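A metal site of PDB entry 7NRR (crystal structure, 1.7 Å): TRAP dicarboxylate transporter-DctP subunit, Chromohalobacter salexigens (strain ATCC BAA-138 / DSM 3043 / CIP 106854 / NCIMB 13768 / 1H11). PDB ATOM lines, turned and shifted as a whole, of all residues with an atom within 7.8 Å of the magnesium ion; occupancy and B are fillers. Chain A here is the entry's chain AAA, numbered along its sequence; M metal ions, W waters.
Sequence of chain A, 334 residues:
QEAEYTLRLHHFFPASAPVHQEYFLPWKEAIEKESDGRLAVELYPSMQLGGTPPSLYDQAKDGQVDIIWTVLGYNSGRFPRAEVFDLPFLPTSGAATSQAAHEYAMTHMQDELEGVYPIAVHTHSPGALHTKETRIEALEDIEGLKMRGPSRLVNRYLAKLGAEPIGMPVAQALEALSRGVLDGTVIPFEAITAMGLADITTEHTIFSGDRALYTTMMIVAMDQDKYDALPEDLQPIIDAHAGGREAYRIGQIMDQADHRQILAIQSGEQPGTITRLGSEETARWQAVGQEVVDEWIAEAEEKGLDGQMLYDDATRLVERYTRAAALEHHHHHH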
ATOM      1  N   ASP A  58     -30.355 -19.396  -1.729  1.00  0.00           N
ATOM      2  CA  ASP A  58     -29.636 -18.172  -1.272  1.00  0.00           C
ATOM      3  C   ASP A  58     -28.711 -18.499  -0.089  1.00  0.00           C
ATOM      4  O   ASP A  58     -27.682 -17.822   0.038  1.00  0.00           O
ATOM      5  CB  ASP A  58     -30.597 -17.027  -0.965  1.00  0.00           C
ATOM      6  CG  ASP A  58     -31.129 -16.316  -2.197  1.00  0.00           C
ATOM      7  OD1 ASP A  58     -30.425 -16.319  -3.219  1.00  0.00           O
ATOM      8  OD2 ASP A  58     -32.229 -15.768  -2.125  1.00  0.00           O
ATOM      9  N   GLN A  59     -29.025 -19.487   0.741  1.00  0.00           N
ATOM     10  CA  GLN A  59     -28.081 -19.891   1.817  1.00  0.00           C
ATOM     11  C   GLN A  59     -26.727 -20.231   1.182  1.00  0.00           C
ATOM     12  O   GLN A  59     -25.710 -19.741   1.675  1.00  0.00           O
ATOM     13  CB  GLN A  59     -28.597 -21.069   2.636  1.00  0.00           C
ATOM     14  CG  GLN A  59     -29.807 -20.720   3.486  1.00  0.00           C
ATOM     15  CD  GLN A  59     -30.119 -21.817   4.470  1.00  0.00           C
ATOM     16  OE1 GLN A  59     -29.243 -22.570   4.892  1.00  0.00           O
ATOM     17  NE2 GLN A  59     -31.385 -21.910   4.835  1.00  0.00           N
ATOM     18  N   ALA A  60     -26.726 -20.979   0.080  1.00  0.00           N
ATOM     19  CA  ALA A  60     -25.485 -21.342  -0.641  1.00  0.00           C
ATOM     20  C   ALA A  60     -24.947 -20.097  -1.352  1.00  0.00           C
ATOM     21  O   ALA A  60     -23.778 -19.763  -1.127  1.00  0.00           O
ATOM     22  CB  ALA A  60     -25.733 -22.466  -1.620  1.00  0.00           C
ATOM     23  N   LYS A  61     -25.755 -19.426  -2.162  1.00  0.00           N
ATOM     24  CA  LYS A  61     -25.309 -18.263  -2.973  1.00  0.00           C
ATOM     25  C   LYS A  61     -24.699 -17.209  -2.052  1.00  0.00           C
ATOM     26  O   LYS A  61     -23.627 -16.699  -2.371  1.00  0.00           O
ATOM     27  CB  LYS A  61     -26.459 -17.676  -3.795  1.00  0.00           C
ATOM     28  CG  LYS A  61     -26.070 -16.471  -4.635  1.00  0.00           C
ATOM     29  CD  LYS A  61     -27.052 -16.172  -5.743  1.00  0.00           C
ATOM     30  CE  LYS A  61     -26.735 -14.896  -6.490  1.00  0.00           C
ATOM     31  NZ  LYS A  61     -26.588 -13.750  -5.571  1.00  0.00           N
ATOM     32  N   ASP A  62     -25.354 -16.928  -0.916  1.00  0.00           N
ATOM     33  CA  ASP A  62     -24.956 -15.850   0.020  1.00  0.00           C
ATOM     34  C   ASP A  62     -23.880 -16.354   0.993  1.00  0.00           C
ATOM     35  O   ASP A  62     -23.303 -15.514   1.681  1.00  0.00           O
ATOM     36  CB  ASP A  62     -26.172 -15.263   0.742  1.00  0.00           C
ATOM     37  CG  ASP A  62     -27.179 -14.589  -0.171  1.00  0.00           C
ATOM     38  OD1 ASP A  62     -26.840 -14.327  -1.345  1.00  0.00           O
ATOM     39  OD2 ASP A  62     -28.281 -14.323   0.295  1.00  0.00           O
ATOM     40  N   GLY A  63     -23.615 -17.664   1.031  1.00  0.00           N
ATOM     41  CA  GLY A  63     -22.497 -18.257   1.781  1.00  0.00           C
ATOM     42  C   GLY A  63     -22.821 -18.546   3.233  1.00  0.00           C
ATOM     43  O   GLY A  63     -21.883 -18.799   4.010  1.00  0.00           O
ATOM     44  N   GLN A  64     -24.099 -18.551   3.622  1.00  0.00           N
ATOM     45  CA  GLN A  64     -24.466 -19.002   4.991  1.00  0.00           C
ATOM     46  C   GLN A  64     -24.048 -20.475   5.158  1.00  0.00           C
ATOM     47  O   GLN A  64     -23.590 -20.850   6.256  1.00  0.00           O
ATOM     48  CB  GLN A  64     -25.960 -18.814   5.250  1.00  0.00           C
ATOM     49  CG  GLN A  64     -26.407 -17.358   5.276  1.00  0.00           C
ATOM     50  CD  GLN A  64     -27.907 -17.250   5.260  1.00  0.00           C
ATOM     51  OE1 GLN A  64     -28.513 -16.778   4.299  1.00  0.00           O
ATOM     52  NE2 GLN A  64     -28.533 -17.738   6.316  1.00  0.00           N
ATOM     53  N   VAL A  65     -24.208 -21.275   4.108  1.00  0.00           N
ATOM     54  CA  VAL A  65     -23.674 -22.662   4.015  1.00  0.00           C
ATOM     55  C   VAL A  65     -22.886 -22.780   2.699  1.00  0.00           C
ATOM     56  O   VAL A  65     -22.941 -21.820   1.903  1.00  0.00           O
ATOM     57  CB  VAL A  65     -24.797 -23.726   4.099  1.00  0.00           C
ATOM     58  CG1 VAL A  65     -25.565 -23.616   5.409  1.00  0.00           C
ATOM     59  CG2 VAL A  65     -25.737 -23.640   2.906  1.00  0.00           C
ATOM     60  N   GLY A 115     -23.434 -16.982  -9.521  1.00  0.00           N
ATOM     61  CA  GLY A 115     -23.219 -17.000  -8.066  1.00  0.00           C
ATOM     62  C   GLY A 115     -23.265 -18.385  -7.450  1.00  0.00           C
ATOM     63  O   GLY A 115     -22.870 -18.508  -6.260  1.00  0.00           O
ATOM     64  N   VAL A 116     -23.664 -19.438  -8.193  1.00  0.00           N
ATOM     65  CA  VAL A 116     -23.554 -20.836  -7.685  1.00  0.00           C
ATOM     66  C   VAL A 116     -22.673 -21.652  -8.635  1.00  0.00           C
ATOM     67  O   VAL A 116     -22.725 -21.447  -9.868  1.00  0.00           O
ATOM     68  CB  VAL A 116     -24.906 -21.534  -7.416  1.00  0.00           C
ATOM     69  CG1 VAL A 116     -25.681 -20.804  -6.344  1.00  0.00           C
ATOM     70  CG2 VAL A 116     -25.747 -21.713  -8.669  1.00  0.00           C
ATOM     71  N   MET A 222     -23.224 -25.130  -5.161  1.00  0.00           N
ATOM     72  CA  MET A 222     -22.154 -24.693  -4.287  1.00  0.00           C
ATOM     73  C   MET A 222     -22.004 -23.180  -4.433  1.00  0.00           C
ATOM     74  O   MET A 222     -22.108 -22.631  -5.531  1.00  0.00           O
ATOM     75  CB  MET A 222     -20.856 -25.437  -4.606  1.00  0.00           C
ATOM     76  CG  MET A 222     -19.768 -25.152  -3.607  1.00  0.00           C
ATOM     77  SD  MET A 222     -18.200 -26.248  -3.973  1.00  0.00           S
ATOM     78  CE  MET A 222     -17.006 -25.783  -2.474  1.00  0.00           C
ATOM     79  N   ASP A 223     -21.761 -22.526  -3.301  1.00  0.00           N
ATOM     80  CA  ASP A 223     -21.384 -21.115  -3.276  1.00  0.00           C
ATOM     81  C   ASP A 223     -20.174 -20.872  -4.202  1.00  0.00           C
ATOM     82  O   ASP A 223     -19.114 -21.442  -3.951  1.00  0.00           O
ATOM     83  CB  ASP A 223     -21.037 -20.710  -1.842  1.00  0.00           C
ATOM     84  CG  ASP A 223     -20.813 -19.222  -1.654  1.00  0.00           C
ATOM     85  OD1 ASP A 223     -20.976 -18.467  -2.645  1.00  0.00           O
ATOM     86  OD2 ASP A 223     -20.500 -18.827  -0.509  1.00  0.00           O
ATOM     87  N   GLN A 224     -20.330 -20.117  -5.281  1.00  0.00           N
ATOM     88  CA  GLN A 224     -19.229 -19.869  -6.250  1.00  0.00           C
ATOM     89  C   GLN A 224     -18.021 -19.270  -5.525  1.00  0.00           C
ATOM     90  O   GLN A 224     -16.894 -19.643  -5.873  1.00  0.00           O
ATOM     91  CB  GLN A 224     -19.667 -18.940  -7.377  1.00  0.00           C
ATOM     92  CG  GLN A 224     -18.598 -18.742  -8.445  1.00  0.00           C
ATOM     93  CD  GLN A 224     -18.388 -19.986  -9.259  1.00  0.00           C
ATOM     94  OE1 GLN A 224     -19.335 -20.606  -9.746  1.00  0.00           O
ATOM     95  NE2 GLN A 224     -17.138 -20.377  -9.408  1.00  0.00           N
ATOM     96  N   ASP A 225     -18.265 -18.381  -4.555  1.00  0.00           N
ATOM     97  CA  ASP A 225     -17.211 -17.718  -3.747  1.00  0.00           C
ATOM     98  C   ASP A 225     -16.412 -18.763  -2.964  1.00  0.00           C
ATOM     99  O   ASP A 225     -15.182 -18.611  -2.880  1.00  0.00           O
ATOM    100  CB  ASP A 225     -17.793 -16.666  -2.796  1.00  0.00           C
ATOM    101  CG  ASP A 225     -18.489 -15.550  -3.540  1.00  0.00           C
ATOM    102  OD1 ASP A 225     -17.830 -14.952  -4.400  1.00  0.00           O
ATOM    103  OD2 ASP A 225     -19.680 -15.336  -3.282  1.00  0.00           O
ATOM    104  N   LYS A 226     -17.069 -19.782  -2.407  1.00  0.00           N
ATOM    105  CA  LYS A 226     -16.353 -20.825  -1.630  1.00  0.00           C
ATOM    106  C   LYS A 226     -15.519 -21.703  -2.584  1.00  0.00           C
ATOM    107  O   LYS A 226     -14.384 -22.051  -2.212  1.00  0.00           O
ATOM    108  CB  LYS A 226     -17.318 -21.680  -0.830  1.00  0.00           C
ATOM    109  CG  LYS A 226     -16.632 -22.673   0.100  1.00  0.00           C
ATOM    110  CD  LYS A 226     -16.059 -22.012   1.338  1.00  0.00           C
ATOM    111  CE  LYS A 226     -15.310 -22.997   2.217  1.00  0.00           C
ATOM    112  NZ  LYS A 226     -15.453 -22.694   3.657  1.00  0.00           N
HETATM  113 MG    MG M   1     -21.556 -16.365  -2.673  1.00  0.00          MG
HETATM  114  O   HOH W   1     -21.023 -16.304  -0.901  1.00  0.00           O
HETATM  115  O   HOH W   2     -21.815 -16.506  -4.803  1.00  0.00           O
HETATM  116  O   HOH W   3     -22.269 -14.250  -2.770  1.00  0.00           O
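Within 4 Å of the magnesium ion: Lys 61, Asp 223 and Asp 225. Along chain A the residues within 4 Å of the magnesium ion span positions 61 to 225. The nearest printed residue that does not touch the magnesium ion is Asp 62 (4.2 Å).
The magnesium ion is bound by water W1 (1.9 Å). O of Lys 61 is bound to the magnesium ion (2.1 Å). Water W2 is bound to the magnesium ion, at 2.2 Å. The side-chain carboxylate (OD1) of Asp 223 binds the magnesium ion. OD2 of Asp 225 is bound to the magnesium ion (2.2 Å). Water W3 binds the magnesium ion (2.2 Å). The magnesium ion has six donor atoms within binding distance.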
